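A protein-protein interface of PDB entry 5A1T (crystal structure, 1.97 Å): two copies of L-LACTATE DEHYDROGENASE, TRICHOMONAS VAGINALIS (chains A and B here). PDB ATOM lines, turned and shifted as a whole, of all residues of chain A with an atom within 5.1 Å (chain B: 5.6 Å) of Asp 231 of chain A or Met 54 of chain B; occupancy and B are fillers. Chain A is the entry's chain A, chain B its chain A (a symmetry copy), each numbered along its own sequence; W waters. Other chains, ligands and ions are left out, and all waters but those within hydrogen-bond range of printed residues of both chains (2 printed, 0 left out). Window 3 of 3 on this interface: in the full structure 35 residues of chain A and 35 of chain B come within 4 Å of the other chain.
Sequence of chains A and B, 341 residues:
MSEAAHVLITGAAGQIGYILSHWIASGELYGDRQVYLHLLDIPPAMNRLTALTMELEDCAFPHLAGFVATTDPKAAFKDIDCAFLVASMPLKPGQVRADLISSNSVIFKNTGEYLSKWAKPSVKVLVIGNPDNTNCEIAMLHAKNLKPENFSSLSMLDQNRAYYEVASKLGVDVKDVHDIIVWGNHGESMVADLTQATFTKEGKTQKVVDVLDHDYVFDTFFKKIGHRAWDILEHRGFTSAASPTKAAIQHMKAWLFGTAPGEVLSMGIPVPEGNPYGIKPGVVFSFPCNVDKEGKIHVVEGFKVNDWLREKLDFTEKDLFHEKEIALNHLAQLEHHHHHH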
ATOM      1  N   HIS A 227      11.028 -28.334  15.275  1.00  0.00           N
ATOM      2  CA  HIS A 227      12.156 -27.467  14.938  1.00  0.00           C
ATOM      3  C   HIS A 227      12.708 -26.716  16.155  1.00  0.00           C
ATOM      4  O   HIS A 227      13.782 -26.116  16.086  1.00  0.00           O
ATOM      5  CB  HIS A 227      11.728 -26.466  13.859  1.00  0.00           C
ATOM      6  CG  HIS A 227      12.827 -25.556  13.402  1.00  0.00           C
ATOM      7  ND1 HIS A 227      13.810 -25.957  12.522  1.00  0.00           N
ATOM      8  CD2 HIS A 227      13.101 -24.265  13.708  1.00  0.00           C
ATOM      9  CE1 HIS A 227      14.638 -24.952  12.303  1.00  0.00           C
ATOM     10  NE2 HIS A 227      14.230 -23.913  13.011  1.00  0.00           N
ATOM     11  N   ARG A 228      11.977 -26.764  17.267  1.00  0.00           N
ATOM     12  CA  ARG A 228      12.300 -25.960  18.445  1.00  0.00           C
ATOM     13  C   ARG A 228      13.749 -26.124  18.911  1.00  0.00           C
ATOM     14  O   ARG A 228      14.429 -25.136  19.186  1.00  0.00           O
ATOM     15  CB  ARG A 228      11.352 -26.317  19.592  1.00  0.00           C
ATOM     16  CG  ARG A 228      11.517 -25.462  20.844  1.00  0.00           C
ATOM     17  CD  ARG A 228      11.215 -23.991  20.579  1.00  0.00           C
ATOM     18  NE  ARG A 228      11.074 -23.239  21.823  1.00  0.00           N
ATOM     19  CZ  ARG A 228      10.678 -21.973  21.900  1.00  0.00           C
ATOM     20  NH1 ARG A 228      10.377 -21.295  20.800  1.00  0.00           N
ATOM     21  NH2 ARG A 228      10.579 -21.382  23.083  1.00  0.00           N
ATOM     22  N   ALA A 229      14.214 -27.367  18.988  1.00  0.00           N
ATOM     23  CA  ALA A 229      15.557 -27.663  19.485  1.00  0.00           C
ATOM     24  C   ALA A 229      16.636 -26.922  18.702  1.00  0.00           C
ATOM     25  O   ALA A 229      17.663 -26.532  19.261  1.00  0.00           O
ATOM     26  CB  ALA A 229      15.815 -29.153  19.431  1.00  0.00           C
ATOM     27  N   TRP A 230      16.400 -26.735  17.409  1.00  0.00           N
ATOM     28  CA  TRP A 230      17.362 -26.061  16.552  1.00  0.00           C
ATOM     29  C   TRP A 230      17.188 -24.548  16.625  1.00  0.00           C
ATOM     30  O   TRP A 230      18.104 -23.795  16.289  1.00  0.00           O
ATOM     31  CB  TRP A 230      17.219 -26.549  15.112  1.00  0.00           C
ATOM     32  CG  TRP A 230      17.145 -28.042  15.009  1.00  0.00           C
ATOM     33  CD1 TRP A 230      16.241 -28.771  14.292  1.00  0.00           C
ATOM     34  CD2 TRP A 230      18.000 -28.992  15.660  1.00  0.00           C
ATOM     35  NE1 TRP A 230      16.485 -30.113  14.448  1.00  0.00           N
ATOM     36  CE2 TRP A 230      17.559 -30.276  15.284  1.00  0.00           C
ATOM     37  CE3 TRP A 230      19.098 -28.881  16.522  1.00  0.00           C
ATOM     38  CZ2 TRP A 230      18.175 -31.441  15.738  1.00  0.00           C
ATOM     39  CZ3 TRP A 230      19.710 -30.039  16.970  1.00  0.00           C
ATOM     40  CH2 TRP A 230      19.246 -31.302  16.577  1.00  0.00           C
ATOM     41  N   ASP A 231      16.016 -24.105  17.068  1.00  0.00           N
ATOM     42  CA  ASP A 231      15.769 -22.681  17.243  1.00  0.00           C
ATOM     43  C   ASP A 231      16.503 -22.192  18.493  1.00  0.00           C
ATOM     44  O   ASP A 231      17.043 -21.085  18.510  1.00  0.00           O
ATOM     45  CB  ASP A 231      14.266 -22.398  17.341  1.00  0.00           C
ATOM     46  CG  ASP A 231      13.898 -20.989  16.894  1.00  0.00           C
ATOM     47  OD1 ASP A 231      14.734 -20.312  16.262  1.00  0.00           O
ATOM     48  OD2 ASP A 231      12.756 -20.562  17.164  1.00  0.00           O
ATOM     49  N   ILE A 232      16.531 -23.027  19.529  1.00  0.00           N
ATOM     50  CA  ILE A 232      17.329 -22.733  20.716  1.00  0.00           C
ATOM     51  C   ILE A 232      18.805 -22.706  20.335  1.00  0.00           C
ATOM     52  O   ILE A 232      19.548 -21.827  20.765  1.00  0.00           O
ATOM     53  CB  ILE A 232      17.090 -23.769  21.850  1.00  0.00           C
ATOM     54  CG1 ILE A 232      15.792 -23.459  22.598  1.00  0.00           C
ATOM     55  CG2 ILE A 232      18.230 -23.767  22.871  1.00  0.00           C
ATOM     56  CD1 ILE A 232      14.544 -23.839  21.854  1.00  0.00           C
ATOM     57  N   LEU A 233      19.221 -23.672  19.519  1.00  0.00           N
ATOM     58  CA  LEU A 233      20.612 -23.766  19.087  1.00  0.00           C
ATOM     59  C   LEU A 233      21.046 -22.505  18.347  1.00  0.00           C
ATOM     60  O   LEU A 233      22.158 -22.016  18.539  1.00  0.00           O
ATOM     61  CB  LEU A 233      20.813 -24.995  18.196  1.00  0.00           C
ATOM     62  CG  LEU A 233      22.204 -25.170  17.581  1.00  0.00           C
ATOM     63  CD1 LEU A 233      23.287 -25.188  18.649  1.00  0.00           C
ATOM     64  CD2 LEU A 233      22.255 -26.444  16.756  1.00  0.00           C
ATOM     65  N   GLU A 234      20.161 -21.983  17.504  1.00  0.00           N
ATOM     66  CA  GLU A 234      20.445 -20.766  16.748  1.00  0.00           C
ATOM     67  C   GLU A 234      20.751 -19.592  17.673  1.00  0.00           C
ATOM     68  O   GLU A 234      21.696 -18.838  17.441  1.00  0.00           O
ATOM     69  CB  GLU A 234      19.263 -20.413  15.839  1.00  0.00           C
ATOM     70  CG  GLU A 234      19.455 -19.125  15.037  1.00  0.00           C
ATOM     71  CD  GLU A 234      18.210 -18.718  14.270  1.00  0.00           C
ATOM     72  OE1 GLU A 234      17.786 -19.474  13.369  1.00  0.00           O
ATOM     73  OE2 GLU A 234      17.660 -17.634  14.565  1.00  0.00           O
ATOM     74  N   HIS A 235      19.950 -19.444  18.723  1.00  0.00           N
ATOM     75  CA  HIS A 235      20.061 -18.294  19.612  1.00  0.00           C
ATOM     76  C   HIS A 235      21.076 -18.510  20.737  1.00  0.00           C
ATOM     77  O   HIS A 235      21.732 -17.563  21.174  1.00  0.00           O
ATOM     78  CB  HIS A 235      18.689 -17.963  20.205  1.00  0.00           C
ATOM     79  CG  HIS A 235      17.674 -17.554  19.184  1.00  0.00           C
ATOM     80  ND1 HIS A 235      16.908 -18.464  18.487  1.00  0.00           N
ATOM     81  CD2 HIS A 235      17.304 -16.331  18.735  1.00  0.00           C
ATOM     82  CE1 HIS A 235      16.107 -17.820  17.658  1.00  0.00           C
ATOM     83  NE2 HIS A 235      16.328 -16.524  17.788  1.00  0.00           N
ATOM     84  N   LEU B  49      20.011 -13.908  25.241  1.00  0.00           N
ATOM     85  CA  LEU B  49      18.884 -13.426  26.028  1.00  0.00           C
ATOM     86  C   LEU B  49      17.587 -14.058  25.529  1.00  0.00           C
ATOM     87  O   LEU B  49      16.759 -14.506  26.321  1.00  0.00           O
ATOM     88  CB  LEU B  49      18.795 -11.900  25.962  1.00  0.00           C
ATOM     89  CG  LEU B  49      17.670 -11.249  26.769  1.00  0.00           C
ATOM     90  CD1 LEU B  49      17.807 -11.559  28.252  1.00  0.00           C
ATOM     91  CD2 LEU B  49      17.653  -9.747  26.534  1.00  0.00           C
ATOM     92  N   THR B  50      17.418 -14.097  24.211  1.00  0.00           N
ATOM     93  CA  THR B  50      16.254 -14.742  23.619  1.00  0.00           C
ATOM     94  C   THR B  50      16.324 -16.241  23.870  1.00  0.00           C
ATOM     95  O   THR B  50      15.316 -16.874  24.187  1.00  0.00           O
ATOM     96  CB  THR B  50      16.160 -14.470  22.109  1.00  0.00           C
ATOM     97  OG1 THR B  50      16.088 -13.057  21.882  1.00  0.00           O
ATOM     98  CG2 THR B  50      14.923 -15.136  21.513  1.00  0.00           C
ATOM     99  N   ALA B  51      17.522 -16.801  23.734  1.00  0.00           N
ATOM    100  CA  ALA B  51      17.742 -18.220  23.988  1.00  0.00           C
ATOM    101  C   ALA B  51      17.324 -18.588  25.406  1.00  0.00           C
ATOM    102  O   ALA B  51      16.806 -19.679  25.646  1.00  0.00           O
ATOM    103  CB  ALA B  51      19.197 -18.578  23.764  1.00  0.00           C
ATOM    104  N   LEU B  52      17.553 -17.673  26.344  1.00  0.00           N
ATOM    105  CA  LEU B  52      17.164 -17.897  27.729  1.00  0.00           C
ATOM    106  C   LEU B  52      15.649 -17.966  27.868  1.00  0.00           C
ATOM    107  O   LEU B  52      15.120 -18.905  28.462  1.00  0.00           O
ATOM    108  CB  LEU B  52      17.716 -16.795  28.638  1.00  0.00           C
ATOM    109  CG  LEU B  52      17.157 -16.800  30.064  1.00  0.00           C
ATOM    110  CD1 LEU B  52      17.367 -18.157  30.715  1.00  0.00           C
ATOM    111  CD2 LEU B  52      17.785 -15.701  30.900  1.00  0.00           C
ATOM    112  N   THR B  53      14.957 -16.970  27.325  1.00  0.00           N
ATOM    113  CA  THR B  53      13.505 -16.911  27.433  1.00  0.00           C
ATOM    114  C   THR B  53      12.868 -18.147  26.819  1.00  0.00           C
ATOM    115  O   THR B  53      11.945 -18.723  27.390  1.00  0.00           O
ATOM    116  CB  THR B  53      12.928 -15.658  26.746  1.00  0.00           C
ATOM    117  OG1 THR B  53      13.343 -15.620  25.374  1.00  0.00           O
ATOM    118  CG2 THR B  53      13.395 -14.402  27.452  1.00  0.00           C
ATOM    119  N   MET B  54      13.376 -18.557  25.662  1.00  0.00           N
ATOM    120  CA  MET B  54      12.850 -19.726  24.969  1.00  0.00           C
ATOM    121  C   MET B  54      12.923 -20.967  25.849  1.00  0.00           C
ATOM    122  O   MET B  54      11.988 -21.763  25.884  1.00  0.00           O
ATOM    123  CB  MET B  54      13.613 -19.963  23.667  1.00  0.00           C
ATOM    124  CG  MET B  54      13.375 -18.891  22.620  1.00  0.00           C
ATOM    125  SD  MET B  54      14.503 -19.034  21.227  1.00  0.00           S
ATOM    126  CE  MET B  54      13.827 -20.469  20.404  1.00  0.00           C
ATOM    127  N   GLU B  55      14.029 -21.127  26.566  1.00  0.00           N
ATOM    128  CA  GLU B  55      14.180 -22.276  27.448  1.00  0.00           C
ATOM    129  C   GLU B  55      13.294 -22.144  28.683  1.00  0.00           C
ATOM    130  O   GLU B  55      12.778 -23.139  29.184  1.00  0.00           O
ATOM    131  CB  GLU B  55      15.638 -22.456  27.859  1.00  0.00           C
ATOM    132  CG  GLU B  55      16.501 -23.037  26.755  1.00  0.00           C
ATOM    133  CD  GLU B  55      17.635 -23.885  27.286  1.00  0.00           C
ATOM    134  OE1 GLU B  55      17.356 -24.873  28.000  1.00  0.00           O
ATOM    135  OE2 GLU B  55      18.805 -23.563  26.992  1.00  0.00           O
ATOM    136  N   LEU B  56      13.119 -20.921  29.174  1.00  0.00           N
ATOM    137  CA  LEU B  56      12.195 -20.687  30.277  1.00  0.00           C
ATOM    138  C   LEU B  56      10.786 -21.089  29.850  1.00  0.00           C
ATOM    139  O   LEU B  56      10.075 -21.769  30.588  1.00  0.00           O
ATOM    140  CB  LEU B  56      12.223 -19.222  30.719  1.00  0.00           C
ATOM    141  CG  LEU B  56      13.493 -18.733  31.422  1.00  0.00           C
ATOM    142  CD1 LEU B  56      13.434 -17.230  31.623  1.00  0.00           C
ATOM    143  CD2 LEU B  56      13.686 -19.438  32.753  1.00  0.00           C
ATOM    144  N   GLU B  57      10.397 -20.670  28.650  1.00  0.00           N
ATOM    145  CA  GLU B  57       9.121 -21.069  28.070  1.00  0.00           C
ATOM    146  C   GLU B  57       9.021 -22.590  27.976  1.00  0.00           C
ATOM    147  O   GLU B  57       7.976 -23.175  28.260  1.00  0.00           O
ATOM    148  CB  GLU B  57       8.944 -20.455  26.678  1.00  0.00           C
ATOM    149  CG  GLU B  57       8.814 -18.942  26.664  1.00  0.00           C
ATOM    150  CD  GLU B  57       8.730 -18.373  25.258  1.00  0.00           C
ATOM    151  OE1 GLU B  57       8.936 -19.137  24.289  1.00  0.00           O
ATOM    152  OE2 GLU B  57       8.458 -17.160  25.124  1.00  0.00           O
ATOM    153  N   ASP B  58      10.125 -23.221  27.582  1.00  0.00           N
ATOM    154  CA  ASP B  58      10.157 -24.658  27.325  1.00  0.00           C
ATOM    155  C   ASP B  58      10.162 -25.504  28.595  1.00  0.00           C
ATOM    156  O   ASP B  58      10.189 -26.734  28.525  1.00  0.00           O
ATOM    157  CB  ASP B  58      11.385 -25.004  26.480  1.00  0.00           C
ATOM    158  CG  ASP B  58      11.269 -24.505  25.053  1.00  0.00           C
ATOM    159  OD1 ASP B  58      10.323 -23.742  24.760  1.00  0.00           O
ATOM    160  OD2 ASP B  58      12.123 -24.878  24.220  1.00  0.00           O
ATOM    161  N   CYS B  59      10.149 -24.850  29.752  1.00  0.00           N
ATOM    162  CA  CYS B  59      10.063 -25.551  31.029  1.00  0.00           C
ATOM    163  C   CYS B  59       8.615 -25.680  31.488  1.00  0.00           C
ATOM    164  O   CYS B  59       8.285 -26.556  32.289  1.00  0.00           O
ATOM    165  CB  CYS B  59      10.879 -24.826  32.098  1.00  0.00           C
ATOM    166  SG  CYS B  59      12.662 -25.071  31.980  1.00  0.00           S
HETATM  167  O   HOH W   1       9.195 -18.650  21.711  1.00  0.00           O
HETATM  168  O   HOH W   2       7.390 -21.097  23.181  1.00  0.00           O
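ND1 of His 235 of chain A lies within hydrogen-bond range of SD of Met 54 of chain B, 3.7 Å away.
The guanidinium group of Arg 228 of chain A lies within salt-bridge range of the side-chain carboxylate of Glu 57 of chain B (3.0 Å).
The guanidinium group (NH2) of Arg 228 of chain A sits at hydrogen-bond distance from the backbone carbonyl oxygen (O) of Met 54 of chain B, 3.2 Å away.
NH2 of Arg 228 of chain A is in salt-bridge range of OD1 of Asp 58 of chain B, at 2.9 Å.
The backbone carbonyl oxygen (O) of Thr 50 of chain B sits at hydrogen-bond distance from the side-chain hydroxyl (OG1) of Thr 53 of chain B, 2.6 Å away.
The backbone carbonyl oxygen (O) of Asp 231 of chain A sits at hydrogen-bond distance from a ring nitrogen (ND1) of His 235 of chain A, at 2.6 Å.
Among the printed residues, merely in contact across the chains: Asp 231 of chain A with Met 54 of chain B, Ile 232 of chain A with Met 54 of chain B, Ile 232 of chain A with Asp 58 of chain B, His 235 of chain A with Thr 50 of chain B and His 235 of chain A with Ala 51 of chain B.
Asp 231 of chain A touches just one residue of chain B: Met 54.
Of the printed residues of chain A, Met 54 of chain B touches Arg 228, Asp 231, Ile 232 and His 235.
Of the printed residues of chain A, Thr 50 of chain B touches His 235 (3.8 Å).
Printed residues of chain B within 4 Å of Ile 232 of chain A: Met 54 (3.7 Å) and Asp 58 (3.5 Å).
Leu 56 of chain B touches none of the printed residues of chain A.
The nearest printed residue of chain B that does not touch Asp 231 of chain A is Ala 51 of chain B (6.2 Å).
The nearest printed residue of chain A that does not touch Met 54 of chain B is Leu 233 of chain A (6.3 Å).
The nearest printed residue of chain A that does not touch Ala 51 of chain B is Ile 232 of chain A (4.4 Å).
Printed residues of chain B that touch a printed residue of chain A: Thr 50, Ala 51, Met 54, Glu 57 and Asp 58.
Hydrophobic or aromatic side chains of chain B that line the printed part of chain A: Ala 51 and Met 54.
Hydrophobic or aromatic side chains of chain A within 4 Å of the printed part of chain B: Ile 232 and His 235.
Along chain A the printed residues that touch a printed residue of chain B span positions 228 to 235.
No position is printed for both chains.
Water W1 lies within hydrogen-bond range of OE1 of Glu 57 of chain B (2.6 Å) and NH1 of Arg 228 of chain A (3.0 Å).
Water W2 lies within hydrogen-bond range of OE1 of Glu 57 of chain B and NH2 of Arg 228 of chain A.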
